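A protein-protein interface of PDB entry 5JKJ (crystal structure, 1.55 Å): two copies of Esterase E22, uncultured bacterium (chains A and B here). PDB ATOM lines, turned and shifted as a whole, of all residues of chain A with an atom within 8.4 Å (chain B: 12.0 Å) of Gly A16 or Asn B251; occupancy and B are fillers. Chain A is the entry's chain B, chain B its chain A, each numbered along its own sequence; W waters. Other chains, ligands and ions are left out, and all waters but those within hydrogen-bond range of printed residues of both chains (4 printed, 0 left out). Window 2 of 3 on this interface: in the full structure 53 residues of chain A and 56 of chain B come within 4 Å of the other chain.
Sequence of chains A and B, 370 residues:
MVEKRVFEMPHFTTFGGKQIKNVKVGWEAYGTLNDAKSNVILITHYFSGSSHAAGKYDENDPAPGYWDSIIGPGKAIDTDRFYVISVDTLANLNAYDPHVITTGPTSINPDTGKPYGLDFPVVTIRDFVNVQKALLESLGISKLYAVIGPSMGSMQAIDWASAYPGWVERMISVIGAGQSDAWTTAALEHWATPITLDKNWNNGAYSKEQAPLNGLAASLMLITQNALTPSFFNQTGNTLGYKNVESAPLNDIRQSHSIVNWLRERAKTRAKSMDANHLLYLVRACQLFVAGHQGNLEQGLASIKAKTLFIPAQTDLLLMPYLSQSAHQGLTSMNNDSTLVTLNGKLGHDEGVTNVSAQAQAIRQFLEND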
ATOM      1  N   PHE A  12      -8.422 -18.193  -1.396  1.00  0.00           N
ATOM      2  CA  PHE A  12      -7.613 -17.818  -0.244  1.00  0.00           C
ATOM      3  C   PHE A  12      -8.381 -18.160   1.023  1.00  0.00           C
ATOM      4  O   PHE A  12      -9.560 -17.812   1.138  1.00  0.00           O
ATOM      5  CB  PHE A  12      -7.296 -16.316  -0.287  1.00  0.00           C
ATOM      6  CG  PHE A  12      -6.483 -15.816   0.880  1.00  0.00           C
ATOM      7  CD1 PHE A  12      -5.102 -15.920   0.867  1.00  0.00           C
ATOM      8  CD2 PHE A  12      -7.092 -15.210   1.964  1.00  0.00           C
ATOM      9  CE1 PHE A  12      -4.337 -15.436   1.927  1.00  0.00           C
ATOM     10  CE2 PHE A  12      -6.337 -14.728   3.025  1.00  0.00           C
ATOM     11  CZ  PHE A  12      -4.962 -14.840   3.007  1.00  0.00           C
ATOM     12  N   THR A  13      -7.711 -18.804   1.977  1.00  0.00           N
ATOM     13  CA  THR A  13      -8.322 -19.140   3.256  1.00  0.00           C
ATOM     14  C   THR A  13      -7.812 -18.178   4.319  1.00  0.00           C
ATOM     15  O   THR A  13      -6.600 -18.034   4.495  1.00  0.00           O
ATOM     16  CB  THR A  13      -8.014 -20.581   3.671  1.00  0.00           C
ATOM     17  OG1 THR A  13      -8.475 -21.487   2.653  1.00  0.00           O
ATOM     18  CG2 THR A  13      -8.718 -20.894   4.982  1.00  0.00           C
ATOM     19  N   THR A  14      -8.736 -17.521   5.016  1.00  0.00           N
ATOM     20  CA  THR A  14      -8.330 -16.562   6.034  1.00  0.00           C
ATOM     21  C   THR A  14      -7.915 -17.266   7.324  1.00  0.00           C
ATOM     22  O   THR A  14      -8.223 -18.438   7.564  1.00  0.00           O
ATOM     23  CB  THR A  14      -9.460 -15.586   6.357  1.00  0.00           C
ATOM     24  OG1 THR A  14     -10.498 -16.290   7.052  1.00  0.00           O
ATOM     25  CG2 THR A  14     -10.031 -14.967   5.098  1.00  0.00           C
ATOM     26  N   PHE A  15      -7.235 -16.503   8.182  1.00  0.00           N
ATOM     27  CA  PHE A  15      -6.853 -17.014   9.492  1.00  0.00           C
ATOM     28  C   PHE A  15      -8.081 -17.410  10.311  1.00  0.00           C
ATOM     29  O   PHE A  15      -8.018 -18.347  11.119  1.00  0.00           O
ATOM     30  CB  PHE A  15      -6.011 -15.946  10.198  1.00  0.00           C
ATOM     31  CG  PHE A  15      -5.437 -16.382  11.505  1.00  0.00           C
ATOM     32  CD1 PHE A  15      -4.354 -17.237  11.554  1.00  0.00           C
ATOM     33  CD2 PHE A  15      -5.959 -15.905  12.694  1.00  0.00           C
ATOM     34  CE1 PHE A  15      -3.818 -17.632  12.763  1.00  0.00           C
ATOM     35  CE2 PHE A  15      -5.421 -16.298  13.910  1.00  0.00           C
ATOM     36  CZ  PHE A  15      -4.355 -17.166  13.945  1.00  0.00           C
ATOM     37  N   GLY A  16      -9.211 -16.728  10.098  1.00  0.00           N
ATOM     38  CA  GLY A  16     -10.463 -17.066  10.742  1.00  0.00           C
ATOM     39  C   GLY A  16     -11.222 -18.224  10.141  1.00  0.00           C
ATOM     40  O   GLY A  16     -12.323 -18.540  10.606  1.00  0.00           O
ATOM     41  N   GLY A  17     -10.673 -18.873   9.118  1.00  0.00           N
ATOM     42  CA  GLY A  17     -11.304 -20.054   8.566  1.00  0.00           C
ATOM     43  C   GLY A  17     -12.335 -19.806   7.491  1.00  0.00           C
ATOM     44  O   GLY A  17     -13.187 -20.676   7.261  1.00  0.00           O
ATOM     45  N   LYS A  18     -12.288 -18.663   6.815  1.00  0.00           N
ATOM     46  CA  LYS A  18     -13.258 -18.327   5.785  1.00  0.00           C
ATOM     47  C   LYS A  18     -12.572 -18.229   4.431  1.00  0.00           C
ATOM     48  O   LYS A  18     -11.341 -18.146   4.332  1.00  0.00           O
ATOM     49  CB  LYS A  18     -13.988 -17.014   6.110  1.00  0.00           C
ATOM     50  CG  LYS A  18     -14.781 -17.101   7.401  1.00  0.00           C
ATOM     51  CD  LYS A  18     -15.891 -16.086   7.454  1.00  0.00           C
ATOM     52  CE  LYS A  18     -16.730 -16.312   8.699  1.00  0.00           C
ATOM     53  NZ  LYS A  18     -16.490 -17.670   9.269  1.00  0.00           N
ATOM     54  N   GLN A  19     -13.381 -18.253   3.382  1.00  0.00           N
ATOM     55  CA  GLN A  19     -12.879 -18.186   2.018  1.00  0.00           C
ATOM     56  C   GLN A  19     -13.018 -16.779   1.461  1.00  0.00           C
ATOM     57  O   GLN A  19     -14.051 -16.124   1.639  1.00  0.00           O
ATOM     58  CB  GLN A  19     -13.627 -19.166   1.112  1.00  0.00           C
ATOM     59  CG  GLN A  19     -13.327 -20.610   1.397  1.00  0.00           C
ATOM     60  CD  GLN A  19     -11.860 -20.927   1.225  1.00  0.00           C
ATOM     61  OE1 GLN A  19     -11.307 -20.819   0.128  1.00  0.00           O
ATOM     62  NE2 GLN A  19     -11.215 -21.316   2.311  1.00  0.00           N
ATOM     63  N   PHE A 120     -18.040  -9.249   4.127  1.00  0.00           N
ATOM     64  CA  PHE A 120     -16.677  -9.660   3.845  1.00  0.00           C
ATOM     65  C   PHE A 120     -16.067 -10.343   5.070  1.00  0.00           C
ATOM     66  O   PHE A 120     -16.364  -9.965   6.206  1.00  0.00           O
ATOM     67  CB  PHE A 120     -15.822  -8.461   3.437  1.00  0.00           C
ATOM     68  CG  PHE A 120     -14.554  -8.863   2.757  1.00  0.00           C
ATOM     69  CD1 PHE A 120     -14.557  -9.216   1.412  1.00  0.00           C
ATOM     70  CD2 PHE A 120     -13.368  -8.941   3.465  1.00  0.00           C
ATOM     71  CE1 PHE A 120     -13.386  -9.616   0.779  1.00  0.00           C
ATOM     72  CE2 PHE A 120     -12.196  -9.346   2.845  1.00  0.00           C
ATOM     73  CZ  PHE A 120     -12.206  -9.680   1.494  1.00  0.00           C
ATOM     74  N   PRO A 121     -15.244 -11.375   4.878  1.00  0.00           N
ATOM     75  CA  PRO A 121     -14.660 -12.074   6.033  1.00  0.00           C
ATOM     76  C   PRO A 121     -13.741 -11.156   6.835  1.00  0.00           C
ATOM     77  O   PRO A 121     -13.051 -10.299   6.276  1.00  0.00           O
ATOM     78  CB  PRO A 121     -13.879 -13.228   5.394  1.00  0.00           C
ATOM     79  CG  PRO A 121     -14.542 -13.443   4.078  1.00  0.00           C
ATOM     80  CD  PRO A 121     -15.006 -12.093   3.615  1.00  0.00           C
ATOM     81  N   VAL A 122     -13.746 -11.349   8.157  1.00  0.00           N
ATOM     82  CA  VAL A 122     -12.792 -10.666   9.028  1.00  0.00           C
ATOM     83  C   VAL A 122     -11.388 -10.949   8.529  1.00  0.00           C
ATOM     84  O   VAL A 122     -11.063 -12.094   8.192  1.00  0.00           O
ATOM     85  CB  VAL A 122     -12.962 -11.140  10.484  1.00  0.00           C
ATOM     86  CG1 VAL A 122     -11.760 -10.722  11.328  1.00  0.00           C
ATOM     87  CG2 VAL A 122     -14.235 -10.577  11.093  1.00  0.00           C
ATOM     88  N   VAL A 123     -10.552  -9.910   8.466  1.00  0.00           N
ATOM     89  CA  VAL A 123      -9.155 -10.080   8.075  1.00  0.00           C
ATOM     90  C   VAL A 123      -8.257  -9.764   9.264  1.00  0.00           C
ATOM     91  O   VAL A 123      -8.625  -9.042  10.198  1.00  0.00           O
ATOM     92  CB  VAL A 123      -8.768  -9.224   6.850  1.00  0.00           C
ATOM     93  CG1 VAL A 123      -9.515  -9.714   5.599  1.00  0.00           C
ATOM     94  CG2 VAL A 123      -9.031  -7.742   7.102  1.00  0.00           C
ATOM     95  N   THR A 124      -7.061 -10.343   9.225  1.00  0.00           N
ATOM     96  CA  THR A 124      -6.055 -10.171  10.257  1.00  0.00           C
ATOM     97  C   THR A 124      -4.743  -9.729   9.627  1.00  0.00           C
ATOM     98  O   THR A 124      -4.538  -9.821   8.411  1.00  0.00           O
ATOM     99  CB  THR A 124      -5.817 -11.464  11.044  1.00  0.00           C
ATOM    100  OG1 THR A 124      -5.323 -12.471  10.150  1.00  0.00           O
ATOM    101  CG2 THR A 124      -7.105 -11.952  11.709  1.00  0.00           C
ATOM    102  N   ARG A 126      -2.210 -11.461   9.915  1.00  0.00           N
ATOM    103  CA  ARG A 126      -1.710 -12.704   9.327  1.00  0.00           C
ATOM    104  C   ARG A 126      -2.183 -12.870   7.889  1.00  0.00           C
ATOM    105  O   ARG A 126      -1.444 -13.387   7.044  1.00  0.00           O
ATOM    106  CB  ARG A 126      -2.160 -13.897  10.164  1.00  0.00           C
ATOM    107  CG  ARG A 126      -1.846 -15.251   9.496  1.00  0.00           C
ATOM    108  CD  ARG A 126      -0.336 -15.426   9.265  1.00  0.00           C
ATOM    109  NE  ARG A 126       0.377 -15.275  10.529  1.00  0.00           N
ATOM    110  CZ  ARG A 126       0.420 -16.207  11.473  1.00  0.00           C
ATOM    111  NH1 ARG A 126      -0.155 -17.391  11.270  1.00  0.00           N
ATOM    112  NH2 ARG A 126       1.041 -15.961  12.618  1.00  0.00           N
ATOM    113  N   ASP A 127      -3.417 -12.456   7.591  1.00  0.00           N
ATOM    114  CA  ASP A 127      -3.910 -12.572   6.221  1.00  0.00           C
ATOM    115  C   ASP A 127      -3.107 -11.702   5.271  1.00  0.00           C
ATOM    116  O   ASP A 127      -2.806 -12.116   4.146  1.00  0.00           O
ATOM    117  CB  ASP A 127      -5.390 -12.213   6.165  1.00  0.00           C
ATOM    118  CG  ASP A 127      -6.227 -13.179   6.956  1.00  0.00           C
ATOM    119  OD1 ASP A 127      -6.048 -14.397   6.767  1.00  0.00           O
ATOM    120  OD2 ASP A 127      -7.048 -12.727   7.776  1.00  0.00           O
ATOM    121  N   ARG A 284     -10.233  -3.887  13.079  1.00  0.00           N
ATOM    122  CA  ARG A 284     -10.370  -5.230  13.639  1.00  0.00           C
ATOM    123  C   ARG A 284      -9.109  -6.063  13.437  1.00  0.00           C
ATOM    124  O   ARG A 284      -8.722  -6.819  14.331  1.00  0.00           O
ATOM    125  CB  ARG A 284     -11.579  -5.939  13.030  1.00  0.00           C
ATOM    126  CG  ARG A 284     -11.766  -7.385  13.483  1.00  0.00           C
ATOM    127  CD  ARG A 284     -11.770  -7.575  15.006  1.00  0.00           C
ATOM    128  NE  ARG A 284     -12.758  -6.703  15.622  1.00  0.00           N
ATOM    129  CZ  ARG A 284     -14.057  -6.976  15.702  1.00  0.00           C
ATOM    130  NH1 ARG A 284     -14.555  -8.114  15.221  1.00  0.00           N
ATOM    131  NH2 ARG A 284     -14.871  -6.084  16.252  1.00  0.00           N
ATOM    132  N   LEU A 288      -6.919  -7.744  16.646  1.00  0.00           N
ATOM    133  CA  LEU A 288      -6.602  -9.165  16.739  1.00  0.00           C
ATOM    134  C   LEU A 288      -5.104  -9.446  16.710  1.00  0.00           C
ATOM    135  O   LEU A 288      -4.708 -10.614  16.771  1.00  0.00           O
ATOM    136  CB  LEU A 288      -7.290  -9.908  15.593  1.00  0.00           C
ATOM    137  CG  LEU A 288      -8.822  -9.952  15.703  1.00  0.00           C
ATOM    138  CD1 LEU A 288      -9.461 -10.297  14.371  1.00  0.00           C
ATOM    139  CD2 LEU A 288      -9.241 -10.925  16.793  1.00  0.00           C
ATOM    140  N   LYS B 243      -7.473 -11.587  25.582  1.00  0.00           N
ATOM    141  CA  LYS B 243      -6.512 -12.226  24.713  1.00  0.00           C
ATOM    142  C   LYS B 243      -6.533 -11.489  23.385  1.00  0.00           C
ATOM    143  O   LYS B 243      -7.521 -10.844  23.025  1.00  0.00           O
ATOM    144  CB  LYS B 243      -6.856 -13.708  24.497  1.00  0.00           C
ATOM    145  CG  LYS B 243      -6.844 -14.556  25.768  1.00  0.00           C
ATOM    146  CD  LYS B 243      -5.428 -14.758  26.287  1.00  0.00           C
ATOM    147  CE  LYS B 243      -5.351 -15.877  27.329  1.00  0.00           C
ATOM    148  NZ  LYS B 243      -6.065 -15.542  28.591  1.00  0.00           N
ATOM    149  N   ASN B 244      -5.425 -11.608  22.662  1.00  0.00           N
ATOM    150  CA  ASN B 244      -5.299 -10.977  21.359  1.00  0.00           C
ATOM    151  C   ASN B 244      -6.247 -11.608  20.347  1.00  0.00           C
ATOM    152  O   ASN B 244      -7.106 -10.932  19.767  1.00  0.00           O
ATOM    153  CB  ASN B 244      -3.839 -11.086  20.918  1.00  0.00           C
ATOM    154  CG  ASN B 244      -2.886 -10.515  21.959  1.00  0.00           C
ATOM    155  OD1 ASN B 244      -2.179 -11.246  22.669  1.00  0.00           O
ATOM    156  ND2 ASN B 244      -2.883  -9.206  22.073  1.00  0.00           N
ATOM    157  N   VAL B 245      -6.119 -12.916  20.146  1.00  0.00           N
ATOM    158  CA  VAL B 245      -6.938 -13.652  19.177  1.00  0.00           C
ATOM    159  C   VAL B 245      -8.107 -14.250  19.954  1.00  0.00           C
ATOM    160  O   VAL B 245      -8.160 -15.440  20.261  1.00  0.00           O
ATOM    161  CB  VAL B 245      -6.126 -14.694  18.410  1.00  0.00           C
ATOM    162  CG1 VAL B 245      -6.947 -15.194  17.234  1.00  0.00           C
ATOM    163  CG2 VAL B 245      -4.816 -14.079  17.913  1.00  0.00           C
ATOM    164  N   GLU B 246      -9.077 -13.396  20.282  1.00  0.00           N
ATOM    165  CA  GLU B 246     -10.322 -13.863  20.877  1.00  0.00           C
ATOM    166  C   GLU B 246     -11.245 -14.405  19.794  1.00  0.00           C
ATOM    167  O   GLU B 246     -11.385 -13.810  18.723  1.00  0.00           O
ATOM    168  CB  GLU B 246     -11.005 -12.734  21.658  1.00  0.00           C
ATOM    169  CG  GLU B 246     -10.272 -12.419  22.951  1.00  0.00           C
ATOM    170  CD  GLU B 246     -10.938 -11.352  23.797  1.00  0.00           C
ATOM    171  OE1 GLU B 246     -12.052 -10.914  23.450  1.00  0.00           O
ATOM    172  OE2 GLU B 246     -10.335 -10.974  24.821  1.00  0.00           O
ATOM    173  N   SER B 247     -11.863 -15.558  20.071  1.00  0.00           N
ATOM    174  CA  SER B 247     -12.599 -16.253  19.020  1.00  0.00           C
ATOM    175  C   SER B 247     -13.762 -15.417  18.496  1.00  0.00           C
ATOM    176  O   SER B 247     -14.009 -15.383  17.284  1.00  0.00           O
ATOM    177  CB  SER B 247     -13.098 -17.606  19.525  1.00  0.00           C
ATOM    178  OG  SER B 247     -13.871 -17.435  20.695  1.00  0.00           O
ATOM    179  N   ALA B 248     -14.495 -14.737  19.384  1.00  0.00           N
ATOM    180  CA  ALA B 248     -15.673 -14.004  18.917  1.00  0.00           C
ATOM    181  C   ALA B 248     -15.309 -12.905  17.925  1.00  0.00           C
ATOM    182  O   ALA B 248     -15.845 -12.912  16.804  1.00  0.00           O
ATOM    183  CB  ALA B 248     -16.481 -13.482  20.111  1.00  0.00           C
ATOM    184  N   PRO B 249     -14.420 -11.950  18.239  1.00  0.00           N
ATOM    185  CA  PRO B 249     -14.087 -10.927  17.233  1.00  0.00           C
ATOM    186  C   PRO B 249     -13.324 -11.462  16.025  1.00  0.00           C
ATOM    187  O   PRO B 249     -13.347 -10.813  14.973  1.00  0.00           O
ATOM    188  CB  PRO B 249     -13.255  -9.906  18.026  1.00  0.00           C
ATOM    189  CG  PRO B 249     -12.709 -10.671  19.182  1.00  0.00           C
ATOM    190  CD  PRO B 249     -13.775 -11.666  19.537  1.00  0.00           C
ATOM    191  N   LEU B 250     -12.663 -12.621  16.130  1.00  0.00           N
ATOM    192  CA  LEU B 250     -12.066 -13.236  14.946  1.00  0.00           C
ATOM    193  C   LEU B 250     -13.131 -13.798  14.010  1.00  0.00           C
ATOM    194  O   LEU B 250     -13.005 -13.701  12.780  1.00  0.00           O
ATOM    195  CB  LEU B 250     -11.107 -14.350  15.357  1.00  0.00           C
ATOM    196  CG  LEU B 250     -10.486 -15.121  14.184  1.00  0.00           C
ATOM    197  CD1 LEU B 250      -9.672 -14.187  13.289  1.00  0.00           C
ATOM    198  CD2 LEU B 250      -9.632 -16.266  14.698  1.00  0.00           C
ATOM    199  N   ASN B 251     -14.184 -14.389  14.576  1.00  0.00           N
ATOM    200  CA  ASN B 251     -15.197 -15.059  13.773  1.00  0.00           C
ATOM    201  C   ASN B 251     -16.255 -14.122  13.219  1.00  0.00           C
ATOM    202  O   ASN B 251     -16.916 -14.473  12.233  1.00  0.00           O
ATOM    203  CB  ASN B 251     -15.877 -16.149  14.604  1.00  0.00           C
ATOM    204  CG  ASN B 251     -14.989 -17.365  14.791  1.00  0.00           C
ATOM    205  OD1 ASN B 251     -14.152 -17.673  13.935  1.00  0.00           O
ATOM    206  ND2 ASN B 251     -15.149 -18.054  15.918  1.00  0.00           N
ATOM    207  N   ASP B 252     -16.420 -12.940  13.806  1.00  0.00           N
ATOM    208  CA  ASP B 252     -17.573 -12.101  13.511  1.00  0.00           C
ATOM    209  C   ASP B 252     -17.180 -10.638  13.640  1.00  0.00           C
ATOM    210  O   ASP B 252     -16.843 -10.186  14.738  1.00  0.00           O
ATOM    211  CB  ASP B 252     -18.716 -12.438  14.471  1.00  0.00           C
ATOM    212  CG  ASP B 252     -20.023 -11.772  14.090  1.00  0.00           C
ATOM    213  OD1 ASP B 252     -20.010 -10.843  13.260  1.00  0.00           O
ATOM    214  OD2 ASP B 252     -21.077 -12.180  14.634  1.00  0.00           O
ATOM    215  N   ILE B 253     -17.258  -9.902  12.526  1.00  0.00           N
ATOM    216  CA  ILE B 253     -16.896  -8.484  12.527  1.00  0.00           C
ATOM    217  C   ILE B 253     -17.750  -7.698  13.513  1.00  0.00           C
ATOM    218  O   ILE B 253     -17.315  -6.664  14.031  1.00  0.00           O
ATOM    219  CB  ILE B 253     -17.004  -7.921  11.090  1.00  0.00           C
ATOM    220  CG1 ILE B 253     -16.536  -6.460  11.021  1.00  0.00           C
ATOM    221  CG2 ILE B 253     -18.448  -8.013  10.585  1.00  0.00           C
ATOM    222  CD1 ILE B 253     -15.055  -6.251  11.369  1.00  0.00           C
ATOM    223  N   ARG B 254     -18.955  -8.181  13.813  1.00  0.00           N
ATOM    224  CA  ARG B 254     -19.868  -7.470  14.695  1.00  0.00           C
ATOM    225  C   ARG B 254     -19.704  -7.834  16.166  1.00  0.00           C
ATOM    226  O   ARG B 254     -20.310  -7.168  17.015  1.00  0.00           O
ATOM    227  CB  ARG B 254     -21.310  -7.721  14.254  1.00  0.00           C
ATOM    228  CG  ARG B 254     -21.591  -7.145  12.873  1.00  0.00           C
ATOM    229  CD  ARG B 254     -23.024  -7.329  12.467  1.00  0.00           C
ATOM    230  NE  ARG B 254     -23.367  -6.504  11.312  1.00  0.00           N
ATOM    231  CZ  ARG B 254     -23.246  -6.887  10.049  1.00  0.00           C
ATOM    232  NH1 ARG B 254     -22.772  -8.097   9.751  1.00  0.00           N
ATOM    233  NH2 ARG B 254     -23.602  -6.045   9.082  1.00  0.00           N
ATOM    234  N   GLN B 255     -18.923  -8.865  16.487  1.00  0.00           N
ATOM    235  CA  GLN B 255     -18.559  -9.137  17.870  1.00  0.00           C
ATOM    236  C   GLN B 255     -17.353  -8.286  18.247  1.00  0.00           C
ATOM    237  O   GLN B 255     -16.623  -7.804  17.383  1.00  0.00           O
ATOM    238  CB  GLN B 255     -18.231 -10.621  18.079  1.00  0.00           C
ATOM    239  CG  GLN B 255     -19.410 -11.573  17.929  1.00  0.00           C
ATOM    240  CD  GLN B 255     -20.200 -11.719  19.209  1.00  0.00           C
ATOM    241  OE1 GLN B 255     -19.865 -11.119  20.229  1.00  0.00           O
ATOM    242  NE2 GLN B 255     -21.261 -12.507  19.161  1.00  0.00           N
ATOM    243  N   SER B 256     -17.135  -8.121  19.553  1.00  0.00           N
ATOM    244  CA  SER B 256     -16.071  -7.267  20.055  1.00  0.00           C
ATOM    245  C   SER B 256     -15.170  -8.042  21.002  1.00  0.00           C
ATOM    246  O   SER B 256     -15.558  -9.073  21.561  1.00  0.00           O
ATOM    247  CB  SER B 256     -16.619  -6.047  20.810  1.00  0.00           C
ATOM    248  OG  SER B 256     -17.478  -5.277  19.995  1.00  0.00           O
ATOM    249  N   HIS B 257     -13.963  -7.502  21.198  1.00  0.00           N
ATOM    250  CA  HIS B 257     -13.081  -7.996  22.242  1.00  0.00           C
ATOM    251  C   HIS B 257     -13.674  -7.773  23.628  1.00  0.00           C
ATOM    252  O   HIS B 257     -14.444  -6.835  23.860  1.00  0.00           O
ATOM    253  CB  HIS B 257     -11.723  -7.297  22.171  1.00  0.00           C
ATOM    254  CG  HIS B 257     -10.770  -7.926  21.208  1.00  0.00           C
ATOM    255  ND1 HIS B 257     -10.781  -7.649  19.859  1.00  0.00           N
ATOM    256  CD2 HIS B 257      -9.761  -8.808  21.405  1.00  0.00           C
ATOM    257  CE1 HIS B 257      -9.820  -8.334  19.265  1.00  0.00           C
ATOM    258  NE2 HIS B 257      -9.182  -9.040  20.182  1.00  0.00           N
ATOM    259  N   SER B 258     -13.258  -8.638  24.557  1.00  0.00           N
ATOM    260  CA  SER B 258     -13.590  -8.501  25.973  1.00  0.00           C
ATOM    261  C   SER B 258     -13.448  -7.073  26.479  1.00  0.00           C
ATOM    262  O   SER B 258     -14.365  -6.539  27.107  1.00  0.00           O
ATOM    263  CB  SER B 258     -12.693  -9.430  26.793  1.00  0.00           C
ATOM    264  OG  SER B 258     -11.328  -9.185  26.506  1.00  0.00           O
ATOM    265  N   ASN B 261     -16.181  -4.846  25.122  1.00  0.00           N
ATOM    266  CA  ASN B 261     -17.456  -5.096  25.793  1.00  0.00           C
ATOM    267  C   ASN B 261     -17.474  -4.476  27.186  1.00  0.00           C
ATOM    268  O   ASN B 261     -18.478  -3.867  27.592  1.00  0.00           O
ATOM    269  CB  ASN B 261     -17.717  -6.596  25.873  1.00  0.00           C
ATOM    270  CG  ASN B 261     -17.985  -7.210  24.518  1.00  0.00           C
ATOM    271  OD1 ASN B 261     -18.551  -6.568  23.640  1.00  0.00           O
ATOM    272  ND2 ASN B 261     -17.579  -8.472  24.342  1.00  0.00           N
HETATM  273  O   HOH W   1     -15.839 -13.260   9.242  1.00  0.00           O
HETATM  274  O   HOH W   2     -17.763  -4.402  15.554  1.00  0.00           O
HETATM  275  O   HOH W   3     -16.546  -3.885  18.030  1.00  0.00           O
HETATM  276  O   HOH W   4     -14.770 -17.443  11.064  1.00  0.00           O
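Phe A15 touches just one residue of chain B: Val B245. Gly A16 touches two residues of chain B. No residue of chain B comes within 4 Å of Gly A17. Val A122 touches just these residues of chain B: Pro B249, Leu B250, Asp B252 and Ile B253. Of the printed residues of chain A, Pro B249 touches Val A122, Arg A284 and Leu A288. Of the printed residues of chain A, Leu B250 touches Gly A16, Val A122, Thr A124 and Leu A288. Of the printed residues of chain A, Asn B251 touches Gly A16 and Lys A18. Printed residues of chain A within 4 Å of His B257: Leu A288 (3.6 Å). The nearest printed residue of chain B that does not touch Leu A288 is Glu B246 (4.1 Å).
The backbone carbonyl oxygen of Pro B249 sits at hydrogen-bond distance from the guanidinium group of Arg A284, at 3.0 Å. The backbone carbonyl oxygen (O) of Asp B252 is in hydrogen-bond range of the guanidinium group (NH1) of Arg A284, 3.1 Å away. The backbone carbonyl oxygen (O) of Ile B253 lies within hydrogen-bond range of the guanidinium group (NH1) of Arg A284 (3.3 Å). NH2 of Arg A284 is in hydrogen-bond range of O of Gln B255 (2.7 Å).
O of Asn B244 is in hydrogen-bond range of NE2 of His B257, 2.8 Å away. The side-chain amide nitrogen of Asn B251 lies within hydrogen-bond range of the backbone carbonyl oxygen of Ser B247, at 3.2 Å. The side-chain carboxylate (OD1) of Asp B252 is in hydrogen-bond range of the backbone NH (N) of Arg B254. The side-chain hydroxyl (OG1) of Thr A14 lies close to the backbone NH (N) of Gly A16. The backbone NH (N) of Phe A15 lies within hydrogen-bond range of the side-chain carboxylate (OD1) of Asp A127 (2.8 Å). OD2 of Asp A127 sits at hydrogen-bond distance from N of Thr A124.
Printed residues of chain B that touch a printed residue of chain A: Asn B244, Val B245, Pro B249, Leu B250, Asn B251, Asp B252, Ile B253, Gln B255 and His B257. Hydrophobic or aromatic side chains of chain B within 4 Å of the printed part of chain A: Val B245, Pro B249, Leu B250, Ile B253 and His B257. Along chain B the printed residues that touch a printed residue of chain A span positions 244 to 257. Among the printed residues, no Asp or Glu carboxylate lies within 4 Å of a Lys or Arg side-chain nitrogen of the other chain.
Water W4 lies within hydrogen-bond range of the side-chain amino group (NZ) of Lys A18 (2.5 Å), the backbone carbonyl oxygen (O) of Gly A16 (2.7 Å) and the side-chain amide oxygen (OD1) of Asn B251 (2.9 Å). Water W3 lies within hydrogen-bond range of the side-chain hydroxyl (OG) of Ser B256 (2.6 Å) and the guanidinium group (NH2) of Arg A284 (3.3 Å). Water W2 lies within hydrogen-bond range of the backbone carbonyl oxygen of Ile B253 and the guanidinium group of Arg A284. Water W1 bridges the backbone NH (N) of Val A122 and the backbone carbonyl oxygen (O) of Asn B251.
Among the printed residues, merely in contact across the chains: Val A122 with Ile B253 (3.4 Å), Val A122 with Leu B250 (3.4 Å), Leu A288 with Asn B244 (3.5 Å), Leu A288 with His B257 (3.6 Å), Leu A288 with Val B245 (3.6 Å), Thr A124 with Leu B250 (3.8 Å), Phe A15 with Val B245 (3.8 Å), Leu A288 with Leu B250 (3.9 Å), Val A122 with Asp B252 (3.9 Å), Gly A16 with Asn B251 (3.9 Å), Gly A16 with Leu B250 (3.9 Å), Leu A288 with Pro B249 (3.97 Å), Val A122 with Pro B249 (3.98 Å) and Lys A18 with Asn B251 (3.99 Å).
No position is printed for both chains.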
